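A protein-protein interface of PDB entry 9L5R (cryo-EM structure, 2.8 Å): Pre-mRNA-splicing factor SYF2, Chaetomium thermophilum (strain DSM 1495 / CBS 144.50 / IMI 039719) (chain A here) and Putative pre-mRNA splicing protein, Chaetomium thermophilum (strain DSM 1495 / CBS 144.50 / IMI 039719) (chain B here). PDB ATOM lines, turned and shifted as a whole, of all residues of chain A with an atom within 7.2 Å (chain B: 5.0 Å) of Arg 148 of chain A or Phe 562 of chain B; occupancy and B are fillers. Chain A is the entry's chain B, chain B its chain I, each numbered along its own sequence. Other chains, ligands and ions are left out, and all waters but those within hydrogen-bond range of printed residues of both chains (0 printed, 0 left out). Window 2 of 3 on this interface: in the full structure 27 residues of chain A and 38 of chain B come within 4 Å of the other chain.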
ATOM      1  N   GLY A 144      11.264  19.118  27.940  1.00  0.00           N
ATOM      2  CA  GLY A 144      11.492  18.465  26.673  1.00  0.00           C
ATOM      3  C   GLY A 144      11.683  16.969  26.826  1.00  0.00           C
ATOM      4  O   GLY A 144      12.002  16.453  27.897  1.00  0.00           O
ATOM      5  N   ASP A 145      11.479  16.257  25.724  1.00  0.00           N
ATOM      6  CA  ASP A 145      11.639  14.810  25.706  1.00  0.00           C
ATOM      7  C   ASP A 145      13.080  14.498  25.328  1.00  0.00           C
ATOM      8  O   ASP A 145      13.499  14.733  24.188  1.00  0.00           O
ATOM      9  CB  ASP A 145      10.652  14.166  24.741  1.00  0.00           C
ATOM     10  CG  ASP A 145      10.575  12.661  24.906  1.00  0.00           C
ATOM     11  OD1 ASP A 145      11.533  11.965  24.510  1.00  0.00           O
ATOM     12  OD2 ASP A 145       9.556  12.176  25.442  1.00  0.00           O
ATOM     13  N   PHE A 146      13.833  13.974  26.295  1.00  0.00           N
ATOM     14  CA  PHE A 146      15.238  13.654  26.077  1.00  0.00           C
ATOM     15  C   PHE A 146      15.397  12.583  25.009  1.00  0.00           C
ATOM     16  O   PHE A 146      16.312  12.649  24.178  1.00  0.00           O
ATOM     17  CB  PHE A 146      15.856  13.212  27.398  1.00  0.00           C
ATOM     18  CG  PHE A 146      17.300  12.849  27.312  1.00  0.00           C
ATOM     19  CD1 PHE A 146      18.251  13.801  27.009  1.00  0.00           C
ATOM     20  CD2 PHE A 146      17.712  11.561  27.579  1.00  0.00           C
ATOM     21  CE1 PHE A 146      19.586  13.464  26.948  1.00  0.00           C
ATOM     22  CE2 PHE A 146      19.042  11.222  27.522  1.00  0.00           C
ATOM     23  CZ  PHE A 146      19.980  12.174  27.206  1.00  0.00           C
ATOM     24  N   GLU A 147      14.490  11.612  24.982  1.00  0.00           N
ATOM     25  CA  GLU A 147      14.616  10.555  23.995  1.00  0.00           C
ATOM     26  C   GLU A 147      14.211  11.007  22.602  1.00  0.00           C
ATOM     27  O   GLU A 147      14.767  10.511  21.625  1.00  0.00           O
ATOM     28  CB  GLU A 147      13.820   9.330  24.428  1.00  0.00           C
ATOM     29  CG  GLU A 147      14.478   8.603  25.580  1.00  0.00           C
ATOM     30  CD  GLU A 147      15.909   8.178  25.275  1.00  0.00           C
ATOM     31  OE1 GLU A 147      16.197   7.779  24.129  1.00  0.00           O
ATOM     32  OE2 GLU A 147      16.757   8.245  26.186  1.00  0.00           O
ATOM     33  N   ARG A 148      13.295  11.967  22.476  1.00  0.00           N
ATOM     34  CA  ARG A 148      13.028  12.552  21.164  1.00  0.00           C
ATOM     35  C   ARG A 148      14.182  13.421  20.677  1.00  0.00           C
ATOM     36  O   ARG A 148      14.558  13.364  19.489  1.00  0.00           O
ATOM     37  CB  ARG A 148      11.741  13.367  21.228  1.00  0.00           C
ATOM     38  CG  ARG A 148      10.500  12.516  21.375  1.00  0.00           C
ATOM     39  CD  ARG A 148       9.244  13.358  21.406  1.00  0.00           C
ATOM     40  NE  ARG A 148       8.888  13.864  20.088  1.00  0.00           N
ATOM     41  CZ  ARG A 148       7.864  14.670  19.850  1.00  0.00           C
ATOM     42  NH1 ARG A 148       7.071  15.086  20.822  1.00  0.00           N
ATOM     43  NH2 ARG A 148       7.632  15.071  18.605  1.00  0.00           N
ATOM     44  N   LYS A 149      14.771  14.202  21.575  1.00  0.00           N
ATOM     45  CA  LYS A 149      15.935  15.000  21.234  1.00  0.00           C
ATOM     46  C   LYS A 149      17.134  14.141  20.842  1.00  0.00           C
ATOM     47  O   LYS A 149      17.966  14.574  20.042  1.00  0.00           O
ATOM     48  CB  LYS A 149      16.289  15.910  22.407  1.00  0.00           C
ATOM     49  CG  LYS A 149      15.302  17.040  22.613  1.00  0.00           C
ATOM     50  CD  LYS A 149      15.614  17.819  23.868  1.00  0.00           C
ATOM     51  CE  LYS A 149      16.907  18.581  23.705  1.00  0.00           C
ATOM     52  NZ  LYS A 149      16.688  19.860  22.979  1.00  0.00           N
ATOM     53  N   ARG A 150      17.245  12.931  21.392  1.00  0.00           N
ATOM     54  CA  ARG A 150      18.282  12.007  20.936  1.00  0.00           C
ATOM     55  C   ARG A 150      17.854  11.253  19.679  1.00  0.00           C
ATOM     56  O   ARG A 150      18.705  10.819  18.879  1.00  0.00           O
ATOM     57  CB  ARG A 150      18.613  11.034  22.059  1.00  0.00           C
ATOM     58  CG  ARG A 150      19.321  11.666  23.227  1.00  0.00           C
ATOM     59  CD  ARG A 150      20.321  10.712  23.822  1.00  0.00           C
ATOM     60  NE  ARG A 150      19.668   9.569  24.441  1.00  0.00           N
ATOM     61  CZ  ARG A 150      20.302   8.632  25.129  1.00  0.00           C
ATOM     62  NH1 ARG A 150      21.613   8.654  25.279  1.00  0.00           N
ATOM     63  NH2 ARG A 150      19.601   7.648  25.680  1.00  0.00           N
ATOM     64  N   ALA A 151      16.538  11.096  19.497  1.00  0.00           N
ATOM     65  CA  ALA A 151      15.992  10.452  18.312  1.00  0.00           C
ATOM     66  C   ALA A 151      16.333  11.240  17.072  1.00  0.00           C
ATOM     67  O   ALA A 151      16.428  10.684  15.975  1.00  0.00           O
ATOM     68  CB  ALA A 151      14.481  10.298  18.444  1.00  0.00           C
ATOM     69  N   TRP A 152      16.551  12.535  17.232  1.00  0.00           N
ATOM     70  CA  TRP A 152      17.078  13.286  16.096  1.00  0.00           C
ATOM     71  C   TRP A 152      18.509  12.896  15.721  1.00  0.00           C
ATOM     72  O   TRP A 152      18.992  13.314  14.669  1.00  0.00           O
ATOM     73  CB  TRP A 152      17.004  14.791  16.350  1.00  0.00           C
ATOM     74  CG  TRP A 152      15.664  15.345  16.045  1.00  0.00           C
ATOM     75  CD1 TRP A 152      14.815  15.946  16.917  1.00  0.00           C
ATOM     76  CD2 TRP A 152      14.989  15.320  14.783  1.00  0.00           C
ATOM     77  NE1 TRP A 152      13.661  16.311  16.279  1.00  0.00           N
ATOM     78  CE2 TRP A 152      13.746  15.937  14.965  1.00  0.00           C
ATOM     79  CE3 TRP A 152      15.323  14.845  13.513  1.00  0.00           C
ATOM     80  CZ2 TRP A 152      12.835  16.088  13.933  1.00  0.00           C
ATOM     81  CZ3 TRP A 152      14.418  14.991  12.496  1.00  0.00           C
ATOM     82  CH2 TRP A 152      13.191  15.608  12.706  1.00  0.00           C
ATOM     83  N   ASP A 153      19.204  12.099  16.547  1.00  0.00           N
ATOM     84  CA  ASP A 153      20.612  11.836  16.268  1.00  0.00           C
ATOM     85  C   ASP A 153      21.001  10.361  16.185  1.00  0.00           C
ATOM     86  O   ASP A 153      22.165  10.070  15.898  1.00  0.00           O
ATOM     87  CB  ASP A 153      21.503  12.485  17.318  1.00  0.00           C
ATOM     88  CG  ASP A 153      21.645  13.962  17.111  1.00  0.00           C
ATOM     89  OD1 ASP A 153      21.602  14.394  15.945  1.00  0.00           O
ATOM     90  OD2 ASP A 153      21.814  14.685  18.110  1.00  0.00           O
ATOM     91  N   TRP A 154      20.097   9.419  16.447  1.00  0.00           N
ATOM     92  CA  TRP A 154      20.443   8.001  16.283  1.00  0.00           C
ATOM     93  C   TRP A 154      20.658   7.631  14.816  1.00  0.00           C
ATOM     94  O   TRP A 154      19.880   8.037  13.954  1.00  0.00           O
ATOM     95  CB  TRP A 154      19.366   7.092  16.867  1.00  0.00           C
ATOM     96  CG  TRP A 154      19.047   7.342  18.285  1.00  0.00           C
ATOM     97  CD1 TRP A 154      17.832   7.639  18.792  1.00  0.00           C
ATOM     98  CD2 TRP A 154      19.949   7.316  19.392  1.00  0.00           C
ATOM     99  NE1 TRP A 154      17.908   7.806  20.144  1.00  0.00           N
ATOM    100  CE2 TRP A 154      19.203   7.611  20.537  1.00  0.00           C
ATOM    101  CE3 TRP A 154      21.312   7.064  19.525  1.00  0.00           C
ATOM    102  CZ2 TRP A 154      19.769   7.665  21.794  1.00  0.00           C
ATOM    103  CZ3 TRP A 154      21.870   7.125  20.766  1.00  0.00           C
ATOM    104  CH2 TRP A 154      21.104   7.423  21.887  1.00  0.00           C
ATOM    105  N   TYR B 558       9.446   2.810  15.087  1.00  0.00           N
ATOM    106  CA  TYR B 558       8.465   3.871  15.286  1.00  0.00           C
ATOM    107  C   TYR B 558       8.984   5.109  16.018  1.00  0.00           C
ATOM    108  O   TYR B 558       8.807   6.214  15.499  1.00  0.00           O
ATOM    109  CB  TYR B 558       7.170   3.430  15.962  1.00  0.00           C
ATOM    110  CG  TYR B 558       6.049   4.315  15.442  1.00  0.00           C
ATOM    111  CD1 TYR B 558       5.379   3.968  14.286  1.00  0.00           C
ATOM    112  CD2 TYR B 558       5.794   5.566  15.974  1.00  0.00           C
ATOM    113  CE1 TYR B 558       4.396   4.764  13.762  1.00  0.00           C
ATOM    114  CE2 TYR B 558       4.820   6.375  15.451  1.00  0.00           C
ATOM    115  CZ  TYR B 558       4.127   5.968  14.342  1.00  0.00           C
ATOM    116  OH  TYR B 558       3.154   6.767  13.805  1.00  0.00           O
ATOM    117  N   PRO B 559       9.577   5.013  17.265  1.00  0.00           N
ATOM    118  CA  PRO B 559       9.632   6.223  18.113  1.00  0.00           C
ATOM    119  C   PRO B 559      10.536   7.334  17.592  1.00  0.00           C
ATOM    120  O   PRO B 559      10.607   8.417  18.178  1.00  0.00           O
ATOM    121  CB  PRO B 559      10.131   5.695  19.466  1.00  0.00           C
ATOM    122  CG  PRO B 559      10.670   4.377  19.211  1.00  0.00           C
ATOM    123  CD  PRO B 559       9.968   3.819  18.039  1.00  0.00           C
ATOM    124  N   VAL B 560      11.225   7.068  16.487  1.00  0.00           N
ATOM    125  CA  VAL B 560      11.965   8.081  15.750  1.00  0.00           C
ATOM    126  C   VAL B 560      11.234   8.406  14.447  1.00  0.00           C
ATOM    127  O   VAL B 560      11.247   9.560  13.943  1.00  0.00           O
ATOM    128  CB  VAL B 560      13.376   7.533  15.518  1.00  0.00           C
ATOM    129  CG1 VAL B 560      14.228   8.569  14.970  1.00  0.00           C
ATOM    130  CG2 VAL B 560      13.945   6.993  16.813  1.00  0.00           C
ATOM    131  N   ALA B 561      10.530   7.409  13.919  1.00  0.00           N
ATOM    132  CA  ALA B 561       9.653   7.630  12.791  1.00  0.00           C
ATOM    133  C   ALA B 561       8.537   8.602  13.124  1.00  0.00           C
ATOM    134  O   ALA B 561       7.954   9.157  12.204  1.00  0.00           O
ATOM    135  CB  ALA B 561       9.063   6.308  12.314  1.00  0.00           C
ATOM    136  N   PHE B 562       8.245   8.861  14.402  1.00  0.00           N
ATOM    137  CA  PHE B 562       7.266   9.899  14.705  1.00  0.00           C
ATOM    138  C   PHE B 562       7.797  11.290  14.406  1.00  0.00           C
ATOM    139  O   PHE B 562       7.035  12.157  13.972  1.00  0.00           O
ATOM    140  CB  PHE B 562       6.813   9.863  16.153  1.00  0.00           C
ATOM    141  CG  PHE B 562       5.842  10.956  16.468  1.00  0.00           C
ATOM    142  CD1 PHE B 562       4.613  10.998  15.842  1.00  0.00           C
ATOM    143  CD2 PHE B 562       6.194  11.995  17.306  1.00  0.00           C
ATOM    144  CE1 PHE B 562       3.730  12.012  16.098  1.00  0.00           C
ATOM    145  CE2 PHE B 562       5.309  13.016  17.561  1.00  0.00           C
ATOM    146  CZ  PHE B 562       4.079  13.020  16.958  1.00  0.00           C
ATOM    147  N   GLU B 563       9.072  11.549  14.693  1.00  0.00           N
ATOM    148  CA  GLU B 563       9.662  12.828  14.310  1.00  0.00           C
ATOM    149  C   GLU B 563       9.583  13.003  12.804  1.00  0.00           C
ATOM    150  O   GLU B 563       9.127  14.050  12.290  1.00  0.00           O
ATOM    151  CB  GLU B 563      11.116  12.881  14.771  1.00  0.00           C
ATOM    152  CG  GLU B 563      11.319  12.786  16.269  1.00  0.00           C
ATOM    153  CD  GLU B 563      10.779  13.988  17.015  1.00  0.00           C
ATOM    154  OE1 GLU B 563      10.787  15.101  16.448  1.00  0.00           O
ATOM    155  OE2 GLU B 563      10.357  13.824  18.177  1.00  0.00           O
ATOM    156  N   LEU B 564       9.951  11.940  12.085  1.00  0.00           N
ATOM    157  CA  LEU B 564       9.817  11.990  10.630  1.00  0.00           C
ATOM    158  C   LEU B 564       8.360  12.137  10.201  1.00  0.00           C
ATOM    159  O   LEU B 564       8.070  12.807   9.210  1.00  0.00           O
ATOM    160  CB  LEU B 564      10.431  10.759   9.976  1.00  0.00           C
ATOM    161  CG  LEU B 564      11.941  10.760   9.771  1.00  0.00           C
ATOM    162  CD1 LEU B 564      12.674  10.465  11.044  1.00  0.00           C
ATOM    163  CD2 LEU B 564      12.297   9.768   8.728  1.00  0.00           C
ATOM    164  N   TRP B 565       7.434  11.538  10.950  1.00  0.00           N
ATOM    165  CA  TRP B 565       6.022  11.579  10.592  1.00  0.00           C
ATOM    166  C   TRP B 565       5.443  12.966  10.794  1.00  0.00           C
ATOM    167  O   TRP B 565       4.591  13.400  10.018  1.00  0.00           O
ATOM    168  CB  TRP B 565       5.229  10.565  11.417  1.00  0.00           C
ATOM    169  CG  TRP B 565       5.034   9.208  10.802  1.00  0.00           C
ATOM    170  CD1 TRP B 565       5.336   8.014  11.369  1.00  0.00           C
ATOM    171  CD2 TRP B 565       4.462   8.907   9.524  1.00  0.00           C
ATOM    172  NE1 TRP B 565       5.012   6.991  10.526  1.00  0.00           N
ATOM    173  CE2 TRP B 565       4.467   7.514   9.387  1.00  0.00           C
ATOM    174  CE3 TRP B 565       3.949   9.681   8.482  1.00  0.00           C
ATOM    175  CZ2 TRP B 565       3.985   6.882   8.260  1.00  0.00           C
ATOM    176  CZ3 TRP B 565       3.475   9.047   7.364  1.00  0.00           C
ATOM    177  CH2 TRP B 565       3.493   7.667   7.260  1.00  0.00           C
ATOM    178  N   ASN B 566       5.870  13.657  11.854  1.00  0.00           N
ATOM    179  CA  ASN B 566       5.522  15.052  12.099  1.00  0.00           C
ATOM    180  C   ASN B 566       5.821  15.874  10.865  1.00  0.00           C
ATOM    181  O   ASN B 566       4.911  16.451  10.238  1.00  0.00           O
ATOM    182  CB  ASN B 566       6.319  15.643  13.261  1.00  0.00           C
ATOM    183  CG  ASN B 566       5.694  15.378  14.594  1.00  0.00           C
ATOM    184  OD1 ASN B 566       4.490  15.191  14.698  1.00  0.00           O
ATOM    185  ND2 ASN B 566       6.504  15.415  15.639  1.00  0.00           N
ATOM    186  N   PHE B 597       1.876   9.187  20.841  1.00  0.00           N
ATOM    187  CA  PHE B 597       1.779   9.924  19.593  1.00  0.00           C
ATOM    188  C   PHE B 597       0.467   9.667  18.871  1.00  0.00           C
ATOM    189  O   PHE B 597       0.138  10.394  17.924  1.00  0.00           O
ATOM    190  CB  PHE B 597       2.946   9.555  18.684  1.00  0.00           C
ATOM    191  CG  PHE B 597       4.288   9.710  19.328  1.00  0.00           C
ATOM    192  CD1 PHE B 597       4.575  10.812  20.110  1.00  0.00           C
ATOM    193  CD2 PHE B 597       5.271   8.761  19.134  1.00  0.00           C
ATOM    194  CE1 PHE B 597       5.813  10.957  20.689  1.00  0.00           C
ATOM    195  CE2 PHE B 597       6.508   8.901  19.708  1.00  0.00           C
ATOM    196  CZ  PHE B 597       6.780  10.000  20.486  1.00  0.00           C
ATOM    197  N   VAL B 600      -1.941  12.671  18.878  1.00  0.00           N
ATOM    198  CA  VAL B 600      -1.649  13.698  17.877  1.00  0.00           C
ATOM    199  C   VAL B 600      -2.045  13.224  16.485  1.00  0.00           C
ATOM    200  O   VAL B 600      -2.686  13.954  15.714  1.00  0.00           O
ATOM    201  CB  VAL B 600      -0.161  14.079  17.926  1.00  0.00           C
ATOM    202  CG1 VAL B 600       0.146  15.151  16.907  1.00  0.00           C
ATOM    203  CG2 VAL B 600       0.218  14.531  19.315  1.00  0.00           C
ATOM    204  N   LEU B 601      -1.662  11.990  16.144  1.00  0.00           N
ATOM    205  CA  LEU B 601      -1.906  11.487  14.795  1.00  0.00           C
ATOM    206  C   LEU B 601      -3.394  11.333  14.520  1.00  0.00           C
ATOM    207  O   LEU B 601      -3.869  11.652  13.427  1.00  0.00           O
ATOM    208  CB  LEU B 601      -1.180  10.162  14.585  1.00  0.00           C
ATOM    209  CG  LEU B 601       0.338  10.290  14.580  1.00  0.00           C
ATOM    210  CD1 LEU B 601       0.959   8.984  14.971  1.00  0.00           C
ATOM    211  CD2 LEU B 601       0.826  10.721  13.224  1.00  0.00           C
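Gly 144 of chain A touches none of the printed residues of chain B. Of chain B, only Phe 562 (3.3 Å), Glu 563 (2.4 Å) and Asn 566 (3.2 Å) come within 4 Å of Arg 148 of chain A. Printed residues of chain B within 4 Å of Ala 151 of chain A: Val 560 (3.2 Å). Printed residues of chain B within 4 Å of Trp 152 of chain A: Glu 563 (3.1 Å). Printed residues of chain A within 4 Å of Val 560 of chain B: Ala 151 (3.2 Å). Of the printed residues of chain A, Phe 562 of chain B touches Arg 148. Trp 565 of chain B touches none of the printed residues of chain A. Of the printed residues of chain A, Asn 566 of chain B touches Arg 148. The nearest residue of chain B that does not touch Arg 148 of chain A is Phe 597 of chain B (4.2 Å). The nearest residue of chain A that does not touch Phe 562 of chain B is Trp 152 of chain A (7.0 Å).
OD1 of Asp 145 of chain A lies within hydrogen-bond range of N of Arg 148 of chain A, at 2.7 Å.
NE of Arg 148 of chain A is in salt-bridge range of OE2 of Glu 563 of chain B (2.4 Å). The side-chain amide nitrogen (ND2) of Asn 566 of chain B sits close to the guanidinium group (NH2) of Arg 148 of chain A, 3.2 Å away. OE1 of Glu 563 of chain B sits at hydrogen-bond distance from NE1 of Trp 152 of chain A (3.1 Å).
Of the 11 printed residues of chain A, 3 touch a printed residue of chain B. Hydrophobic or aromatic side chains of chain B that line the printed part of chain A: Val 560 and Phe 562. Among the printed residues, 5 pairs touch across the chains. Among the printed residues, Asp or Glu carboxylates within 4 Å of a Lys or Arg side-chain nitrogen of the other chain: Arg 148 of chain A with Glu 563 of chain B.
Among the printed residues, merely in contact across the chains: Ala 151 of chain A with Val 560 of chain B (3.2 Å) and Arg 148 of chain A with Phe 562 of chain B (3.3 Å).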
